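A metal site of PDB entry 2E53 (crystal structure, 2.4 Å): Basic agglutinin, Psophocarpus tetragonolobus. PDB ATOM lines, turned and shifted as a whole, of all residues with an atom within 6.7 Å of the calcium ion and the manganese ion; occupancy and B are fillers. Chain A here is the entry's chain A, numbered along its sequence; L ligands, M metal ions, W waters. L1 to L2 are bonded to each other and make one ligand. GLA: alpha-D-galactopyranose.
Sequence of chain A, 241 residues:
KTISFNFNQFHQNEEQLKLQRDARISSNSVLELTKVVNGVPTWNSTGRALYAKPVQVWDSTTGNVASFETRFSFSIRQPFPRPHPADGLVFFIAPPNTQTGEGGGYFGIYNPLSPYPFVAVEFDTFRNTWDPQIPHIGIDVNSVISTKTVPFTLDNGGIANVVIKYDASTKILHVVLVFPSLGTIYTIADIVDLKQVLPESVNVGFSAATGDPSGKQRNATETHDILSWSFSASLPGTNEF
The calcium ion is bound by water W3 (2.3 Å), O of Phe 126 (2.3 Å), OD2 of Asp 131 (2.4 Å), water W1 (2.4 Å), OD1 of Asp 124 (2.5 Å), OD2 of Asp 124 (2.5 Å) and OD1 of Asn 128 (2.8 Å).
The calcium ion has seven donor atoms within binding distance.
Within 4 Å of the manganese ion: Glu 122, Asp 124, Asp 131 and His 136.
The nearest printed residue that does not touch the manganese ion is Ser 146 (4.2 Å).
The side-chain amide nitrogen (ND2) of Asn 128 sits at hydrogen-bond distance from an oxygen (O3) of GLA L2 (3.4 Å).
The backbone NH (N) of Gly 105 sits at hydrogen-bond distance from an oxygen (O3) of GLA L2, at 2.7 Å.
OD1 of Asp 87 sits at hydrogen-bond distance from O4 of GLA L2, 2.6 Å away.
Water W1 lies within hydrogen-bond range of O of Gly 105 (2.8 Å) and NE1 of Trp 130 (3.3 Å).
Water W2 lies within hydrogen-bond range of O of Val 144 (2.7 Å), OE1 of Glu 122 (2.7 Å) and NE1 of Trp 130 (3.5 Å).
The manganese ion is bound by the side-chain carboxylate (OD1) of Asp 131 (2.2 Å), the side-chain carboxylate (OE2) of Glu 122 (2.2 Å), the side-chain carboxylate (OD2) of Asp 124 (2.2 Å), water W2 (2.3 Å), water W4 (2.3 Å) and a ring nitrogen (NE2) of His 136 (2.5 Å).
O of Asp 131 is in hydrogen-bond range of NE of Arg 127.
OD2 of Asp 140 sits close to OE1 of Glu 122 (2.5 Å).
The backbone carbonyl oxygen (O) of Gly 138 sits at hydrogen-bond distance from the backbone NH (N) of Glu 122 (2.8 Å).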
ATOM      1  N   ASP A  87     -29.557  -6.414   7.941  1.00  0.00           N
ATOM      2  CA  ASP A  87     -28.730  -5.622   8.876  1.00  0.00           C
ATOM      3  C   ASP A  87     -29.456  -4.372   9.380  1.00  0.00           C
ATOM      4  O   ASP A  87     -29.183  -3.855  10.464  1.00  0.00           O
ATOM      5  CB  ASP A  87     -27.428  -5.173   8.190  1.00  0.00           C
ATOM      6  CG  ASP A  87     -26.281  -6.160   8.395  1.00  0.00           C
ATOM      7  OD1 ASP A  87     -26.019  -6.977   7.477  1.00  0.00           O
ATOM      8  OD2 ASP A  87     -25.655  -6.118   9.480  1.00  0.00           O
ATOM      9  N   GLY A 104     -23.737  -5.041   4.533  1.00  0.00           N
ATOM     10  CA  GLY A 104     -23.709  -5.469   5.928  1.00  0.00           C
ATOM     11  C   GLY A 104     -23.965  -4.347   6.917  1.00  0.00           C
ATOM     12  O   GLY A 104     -24.860  -3.505   6.702  1.00  0.00           O
ATOM     13  N   GLY A 105     -23.173  -4.318   7.990  1.00  0.00           N
ATOM     14  CA  GLY A 105     -23.300  -3.318   9.038  1.00  0.00           C
ATOM     15  C   GLY A 105     -23.020  -1.922   8.592  1.00  0.00           C
ATOM     16  O   GLY A 105     -23.203  -0.990   9.372  1.00  0.00           O
ATOM     17  N   TYR A 106     -22.583  -1.754   7.348  1.00  0.00           N
ATOM     18  CA  TYR A 106     -22.308  -0.410   6.809  1.00  0.00           C
ATOM     19  C   TYR A 106     -23.504   0.136   5.996  1.00  0.00           C
ATOM     20  O   TYR A 106     -23.435   1.224   5.422  1.00  0.00           O
ATOM     21  CB  TYR A 106     -21.051  -0.439   5.951  1.00  0.00           C
ATOM     22  CG  TYR A 106     -19.811  -0.737   6.733  1.00  0.00           C
ATOM     23  CD1 TYR A 106     -19.389   0.125   7.747  1.00  0.00           C
ATOM     24  CD2 TYR A 106     -19.056  -1.874   6.472  1.00  0.00           C
ATOM     25  CE1 TYR A 106     -18.228  -0.148   8.487  1.00  0.00           C
ATOM     26  CE2 TYR A 106     -17.899  -2.156   7.214  1.00  0.00           C
ATOM     27  CZ  TYR A 106     -17.493  -1.292   8.215  1.00  0.00           C
ATOM     28  OH  TYR A 106     -16.342  -1.572   8.915  1.00  0.00           O
ATOM     29  N   PHE A 107     -24.563  -0.665   5.934  1.00  0.00           N
ATOM     30  CA  PHE A 107     -25.818  -0.297   5.288  1.00  0.00           C
ATOM     31  C   PHE A 107     -25.738   0.174   3.858  1.00  0.00           C
ATOM     32  O   PHE A 107     -26.742   0.615   3.306  1.00  0.00           O
ATOM     33  CB  PHE A 107     -26.519   0.816   6.105  1.00  0.00           C
ATOM     34  CG  PHE A 107     -26.589   0.545   7.580  1.00  0.00           C
ATOM     35  CD1 PHE A 107     -27.381  -0.475   8.077  1.00  0.00           C
ATOM     36  CD2 PHE A 107     -25.892   1.347   8.477  1.00  0.00           C
ATOM     37  CE1 PHE A 107     -27.494  -0.685   9.478  1.00  0.00           C
ATOM     38  CE2 PHE A 107     -25.991   1.146   9.848  1.00  0.00           C
ATOM     39  CZ  PHE A 107     -26.796   0.135  10.362  1.00  0.00           C
ATOM     40  N   GLU A 122     -30.156   5.589  11.604  1.00  0.00           N
ATOM     41  CA  GLU A 122     -30.237   4.163  11.375  1.00  0.00           C
ATOM     42  C   GLU A 122     -31.247   3.442  12.254  1.00  0.00           C
ATOM     43  O   GLU A 122     -31.560   3.849  13.366  1.00  0.00           O
ATOM     44  CB  GLU A 122     -28.863   3.514  11.585  1.00  0.00           C
ATOM     45  CG  GLU A 122     -28.379   3.691  13.008  1.00  0.00           C
ATOM     46  CD  GLU A 122     -27.137   2.877  13.342  1.00  0.00           C
ATOM     47  OE1 GLU A 122     -26.104   3.019  12.635  1.00  0.00           O
ATOM     48  OE2 GLU A 122     -27.201   2.120  14.320  1.00  0.00           O
ATOM     49  N   ASP A 124     -31.031  -0.089  13.188  1.00  0.00           N
ATOM     50  CA  ASP A 124     -30.095  -1.192  13.216  1.00  0.00           C
ATOM     51  C   ASP A 124     -30.661  -2.447  13.835  1.00  0.00           C
ATOM     52  O   ASP A 124     -31.090  -2.437  14.981  1.00  0.00           O
ATOM     53  CB  ASP A 124     -28.854  -0.751  13.989  1.00  0.00           C
ATOM     54  CG  ASP A 124     -27.636  -1.560  13.642  1.00  0.00           C
ATOM     55  OD1 ASP A 124     -27.764  -2.753  13.248  1.00  0.00           O
ATOM     56  OD2 ASP A 124     -26.559  -1.011  13.794  1.00  0.00           O
ATOM     57  N   THR A 125     -30.611  -3.538  13.066  1.00  0.00           N
ATOM     58  CA  THR A 125     -31.156  -4.818  13.520  1.00  0.00           C
ATOM     59  C   THR A 125     -30.114  -5.913  13.853  1.00  0.00           C
ATOM     60  O   THR A 125     -30.472  -6.969  14.409  1.00  0.00           O
ATOM     61  CB  THR A 125     -32.136  -5.365  12.461  1.00  0.00           C
ATOM     62  OG1 THR A 125     -31.489  -5.420  11.189  1.00  0.00           O
ATOM     63  CG2 THR A 125     -33.365  -4.470  12.393  1.00  0.00           C
ATOM     64  N   PHE A 126     -28.849  -5.676  13.493  1.00  0.00           N
ATOM     65  CA  PHE A 126     -27.781  -6.635  13.757  1.00  0.00           C
ATOM     66  C   PHE A 126     -26.702  -6.013  14.627  1.00  0.00           C
ATOM     67  O   PHE A 126     -26.228  -4.904  14.356  1.00  0.00           O
ATOM     68  CB  PHE A 126     -27.139  -7.101  12.467  1.00  0.00           C
ATOM     69  CG  PHE A 126     -26.035  -8.102  12.694  1.00  0.00           C
ATOM     70  CD1 PHE A 126     -26.330  -9.452  12.909  1.00  0.00           C
ATOM     71  CD2 PHE A 126     -24.697  -7.692  12.697  1.00  0.00           C
ATOM     72  CE1 PHE A 126     -25.309 -10.386  13.126  1.00  0.00           C
ATOM     73  CE2 PHE A 126     -23.673  -8.617  12.912  1.00  0.00           C
ATOM     74  CZ  PHE A 126     -23.970  -9.945  13.127  1.00  0.00           C
ATOM     75  N   ARG A 127     -26.312  -6.722  15.681  1.00  0.00           N
ATOM     76  CA  ARG A 127     -25.296  -6.183  16.567  1.00  0.00           C
ATOM     77  C   ARG A 127     -23.864  -6.437  16.123  1.00  0.00           C
ATOM     78  O   ARG A 127     -23.345  -7.514  16.297  1.00  0.00           O
ATOM     79  CB  ARG A 127     -25.488  -6.718  17.990  1.00  0.00           C
ATOM     80  CG  ARG A 127     -24.564  -6.031  18.976  1.00  0.00           C
ATOM     81  CD  ARG A 127     -24.843  -6.427  20.418  1.00  0.00           C
ATOM     82  NE  ARG A 127     -24.035  -5.611  21.338  1.00  0.00           N
ATOM     83  CZ  ARG A 127     -24.120  -5.667  22.657  1.00  0.00           C
ATOM     84  NH1 ARG A 127     -24.958  -6.523  23.240  1.00  0.00           N
ATOM     85  NH2 ARG A 127     -23.364  -4.866  23.402  1.00  0.00           N
ATOM     86  N   ASN A 128     -23.242  -5.432  15.521  1.00  0.00           N
ATOM     87  CA  ASN A 128     -21.860  -5.538  15.089  1.00  0.00           C
ATOM     88  C   ASN A 128     -20.985  -5.323  16.328  1.00  0.00           C
ATOM     89  O   ASN A 128     -21.488  -5.115  17.439  1.00  0.00           O
ATOM     90  CB  ASN A 128     -21.539  -4.482  14.038  1.00  0.00           C
ATOM     91  CG  ASN A 128     -22.008  -4.873  12.637  1.00  0.00           C
ATOM     92  OD1 ASN A 128     -23.086  -4.470  12.192  1.00  0.00           O
ATOM     93  ND2 ASN A 128     -21.190  -5.654  11.925  1.00  0.00           N
ATOM     94  N   TRP A 130     -19.175  -2.826  17.094  1.00  0.00           N
ATOM     95  CA  TRP A 130     -19.291  -1.436  17.545  1.00  0.00           C
ATOM     96  C   TRP A 130     -20.691  -1.051  18.041  1.00  0.00           C
ATOM     97  O   TRP A 130     -20.895   0.098  18.444  1.00  0.00           O
ATOM     98  CB  TRP A 130     -18.887  -0.512  16.409  1.00  0.00           C
ATOM     99  CG  TRP A 130     -19.712  -0.730  15.179  1.00  0.00           C
ATOM    100  CD1 TRP A 130     -21.006  -0.333  14.963  1.00  0.00           C
ATOM    101  CD2 TRP A 130     -19.319  -1.448  13.988  1.00  0.00           C
ATOM    102  NE1 TRP A 130     -21.449  -0.757  13.730  1.00  0.00           N
ATOM    103  CE2 TRP A 130     -20.429  -1.439  13.112  1.00  0.00           C
ATOM    104  CE3 TRP A 130     -18.144  -2.083  13.591  1.00  0.00           C
ATOM    105  CZ2 TRP A 130     -20.389  -2.054  11.850  1.00  0.00           C
ATOM    106  CZ3 TRP A 130     -18.097  -2.688  12.335  1.00  0.00           C
ATOM    107  CH2 TRP A 130     -19.215  -2.670  11.485  1.00  0.00           C
ATOM    108  N   ASP A 131     -21.633  -1.999  18.012  1.00  0.00           N
ATOM    109  CA  ASP A 131     -23.017  -1.749  18.411  1.00  0.00           C
ATOM    110  C   ASP A 131     -23.437  -2.146  19.800  1.00  0.00           C
ATOM    111  O   ASP A 131     -22.869  -3.053  20.393  1.00  0.00           O
ATOM    112  CB  ASP A 131     -24.015  -2.485  17.488  1.00  0.00           C
ATOM    113  CG  ASP A 131     -24.150  -1.875  16.129  1.00  0.00           C
ATOM    114  OD1 ASP A 131     -24.163  -0.632  16.007  1.00  0.00           O
ATOM    115  OD2 ASP A 131     -24.268  -2.650  15.159  1.00  0.00           O
ATOM    116  N   PRO A 132     -24.460  -1.462  20.331  1.00  0.00           N
ATOM    117  CA  PRO A 132     -25.044  -1.719  21.643  1.00  0.00           C
ATOM    118  C   PRO A 132     -26.188  -2.685  21.314  1.00  0.00           C
ATOM    119  O   PRO A 132     -26.334  -3.085  20.169  1.00  0.00           O
ATOM    120  CB  PRO A 132     -25.561  -0.345  22.080  1.00  0.00           C
ATOM    121  CG  PRO A 132     -25.946   0.272  20.786  1.00  0.00           C
ATOM    122  CD  PRO A 132     -24.786  -0.089  19.893  1.00  0.00           C
ATOM    123  N   ILE A 134     -29.483  -4.539  20.125  1.00  0.00           N
ATOM    124  CA  ILE A 134     -30.351  -4.228  18.982  1.00  0.00           C
ATOM    125  C   ILE A 134     -31.745  -4.798  19.265  1.00  0.00           C
ATOM    126  O   ILE A 134     -31.908  -5.660  20.122  1.00  0.00           O
ATOM    127  CB  ILE A 134     -29.819  -4.795  17.620  1.00  0.00           C
ATOM    128  CG1 ILE A 134     -29.450  -6.293  17.725  1.00  0.00           C
ATOM    129  CG2 ILE A 134     -28.629  -3.988  17.160  1.00  0.00           C
ATOM    130  CD1 ILE A 134     -30.672  -7.231  17.822  1.00  0.00           C
ATOM    131  N   HIS A 136     -31.954  -0.900  17.538  1.00  0.00           N
ATOM    132  CA  HIS A 136     -31.815   0.430  18.115  1.00  0.00           C
ATOM    133  C   HIS A 136     -31.801   1.498  17.023  1.00  0.00           C
ATOM    134  O   HIS A 136     -31.490   1.229  15.856  1.00  0.00           O
ATOM    135  CB  HIS A 136     -30.536   0.544  18.965  1.00  0.00           C
ATOM    136  CG  HIS A 136     -29.258   0.277  18.218  1.00  0.00           C
ATOM    137  ND1 HIS A 136     -28.510  -0.858  18.407  1.00  0.00           N
ATOM    138  CD2 HIS A 136     -28.618   1.009  17.262  1.00  0.00           C
ATOM    139  CE1 HIS A 136     -27.451  -0.824  17.597  1.00  0.00           C
ATOM    140  NE2 HIS A 136     -27.497   0.292  16.898  1.00  0.00           N
ATOM    141  N   ILE A 137     -32.177   2.711  17.427  1.00  0.00           N
ATOM    142  CA  ILE A 137     -32.154   3.844  16.526  1.00  0.00           C
ATOM    143  C   ILE A 137     -30.815   4.499  16.798  1.00  0.00           C
ATOM    144  O   ILE A 137     -30.339   4.515  17.937  1.00  0.00           O
ATOM    145  CB  ILE A 137     -33.256   4.869  16.854  1.00  0.00           C
ATOM    146  CG1 ILE A 137     -34.619   4.188  16.942  1.00  0.00           C
ATOM    147  CG2 ILE A 137     -33.284   5.922  15.784  1.00  0.00           C
ATOM    148  CD1 ILE A 137     -35.734   5.132  17.317  1.00  0.00           C
ATOM    149  N   GLY A 138     -30.200   5.037  15.759  1.00  0.00           N
ATOM    150  CA  GLY A 138     -28.919   5.669  15.949  1.00  0.00           C
ATOM    151  C   GLY A 138     -28.743   6.861  15.047  1.00  0.00           C
ATOM    152  O   GLY A 138     -29.271   6.912  13.938  1.00  0.00           O
ATOM    153  N   ASP A 140     -25.970   8.792  13.090  1.00  0.00           N
ATOM    154  CA  ASP A 140     -24.635   8.601  12.555  1.00  0.00           C
ATOM    155  C   ASP A 140     -24.091   9.787  11.797  1.00  0.00           C
ATOM    156  O   ASP A 140     -24.736  10.316  10.917  1.00  0.00           O
ATOM    157  CB  ASP A 140     -24.611   7.371  11.622  1.00  0.00           C
ATOM    158  CG  ASP A 140     -25.151   6.116  12.272  1.00  0.00           C
ATOM    159  OD1 ASP A 140     -25.153   6.027  13.520  1.00  0.00           O
ATOM    160  OD2 ASP A 140     -25.560   5.200  11.546  1.00  0.00           O
ATOM    161  N   VAL A 144     -20.611   4.728  11.154  1.00  0.00           N
ATOM    162  CA  VAL A 144     -21.740   3.927  11.585  1.00  0.00           C
ATOM    163  C   VAL A 144     -21.645   3.663  13.079  1.00  0.00           C
ATOM    164  O   VAL A 144     -22.472   2.952  13.656  1.00  0.00           O
ATOM    165  CB  VAL A 144     -21.910   2.660  10.649  1.00  0.00           C
ATOM    166  CG1 VAL A 144     -21.851   3.133   9.195  1.00  0.00           C
ATOM    167  CG2 VAL A 144     -20.816   1.640  10.871  1.00  0.00           C
ATOM    168  N   ILE A 145     -20.657   4.277  13.705  1.00  0.00           N
ATOM    169  CA  ILE A 145     -20.505   4.181  15.168  1.00  0.00           C
ATOM    170  C   ILE A 145     -21.264   5.401  15.680  1.00  0.00           C
ATOM    171  O   ILE A 145     -20.705   6.486  15.828  1.00  0.00           O
ATOM    172  CB  ILE A 145     -19.020   4.259  15.597  1.00  0.00           C
ATOM    173  CG1 ILE A 145     -18.240   3.101  14.968  1.00  0.00           C
ATOM    174  CG2 ILE A 145     -18.920   4.153  17.086  1.00  0.00           C
ATOM    175  CD1 ILE A 145     -16.770   3.146  15.240  1.00  0.00           C
ATOM    176  N   SER A 146     -22.568   5.195  15.900  1.00  0.00           N
ATOM    177  CA  SER A 146     -23.513   6.251  16.338  1.00  0.00           C
ATOM    178  C   SER A 146     -23.041   7.158  17.470  1.00  0.00           C
ATOM    179  O   SER A 146     -22.339   6.744  18.368  1.00  0.00           O
ATOM    180  CB  SER A 146     -24.834   5.602  16.749  1.00  0.00           C
ATOM    181  OG  SER A 146     -25.311   4.747  15.738  1.00  0.00           O
ATOM    182  N   THR A 149     -27.667   6.491  20.625  1.00  0.00           N
ATOM    183  CA  THR A 149     -28.545   5.388  20.256  1.00  0.00           C
ATOM    184  C   THR A 149     -29.637   5.225  21.295  1.00  0.00           C
ATOM    185  O   THR A 149     -29.528   5.714  22.405  1.00  0.00           O
ATOM    186  CB  THR A 149     -27.808   4.037  20.156  1.00  0.00           C
ATOM    187  OG1 THR A 149     -27.241   3.711  21.426  1.00  0.00           O
ATOM    188  CG2 THR A 149     -26.715   4.072  19.083  1.00  0.00           C
HETATM  189  C1  GLA L   1     -17.487 -11.990  10.546  1.00  0.00           C
HETATM  190  C2  GLA L   1     -18.747 -11.339   9.911  1.00  0.00           C
HETATM  191  C3  GLA L   1     -19.536 -10.544  10.988  1.00  0.00           C
HETATM  192  C4  GLA L   1     -19.875 -11.483  12.150  1.00  0.00           C
HETATM  193  C5  GLA L   1     -18.573 -12.099  12.716  1.00  0.00           C
HETATM  194  C6  GLA L   1     -18.895 -13.058  13.859  1.00  0.00           C
HETATM  195  O1  GLA L   1     -16.584 -11.009  10.980  1.00  0.00           O
HETATM  196  O2  GLA L   1     -18.351 -10.459   8.850  1.00  0.00           O
HETATM  197  O3  GLA L   1     -20.771  -9.946  10.480  1.00  0.00           O
HETATM  198  O4  GLA L   1     -20.759 -12.493  11.708  1.00  0.00           O
HETATM  199  O5  GLA L   1     -17.868 -12.840  11.664  1.00  0.00           O
HETATM  200  O6  GLA L   1     -17.709 -13.644  14.402  1.00  0.00           O
HETATM  201  C1  GLA L   2     -21.134  -9.913   9.103  1.00  0.00           C
HETATM  202  C2  GLA L   2     -21.497  -8.454   8.709  1.00  0.00           C
HETATM  203  C3  GLA L   2     -22.737  -8.027   9.546  1.00  0.00           C
HETATM  204  C4  GLA L   2     -23.900  -8.973   9.235  1.00  0.00           C
HETATM  205  C5  GLA L   2     -23.462 -10.430   9.559  1.00  0.00           C
HETATM  206  C6  GLA L   2     -24.575 -11.420   9.217  1.00  0.00           C
HETATM  207  O2  GLA L   2     -20.397  -7.584   8.979  1.00  0.00           O
HETATM  208  O3  GLA L   2     -23.110  -6.687   9.268  1.00  0.00           O
HETATM  209  O4  GLA L   2     -24.259  -8.868   7.850  1.00  0.00           O
HETATM  210  O5  GLA L   2     -22.256 -10.782   8.810  1.00  0.00           O
HETATM  211  O6  GLA L   2     -24.186 -12.749   9.520  1.00  0.00           O
HETATM  212 CA    CA M   1     -25.329  -3.130  13.106  1.00  0.00          CA
HETATM  213 MN    MN M   2     -25.770   0.606  15.123  1.00  0.00          MN
HETATM  214  O   HOH W   1     -24.100  -1.372  11.953  1.00  0.00           O
HETATM  215  O   HOH W   2     -24.370   1.116  13.379  1.00  0.00           O
HETATM  216  O   HOH W   3     -26.261  -3.965  11.177  1.00  0.00           O
HETATM  217  O   HOH W   4     -24.798   2.263  16.404  1.00  0.00           O
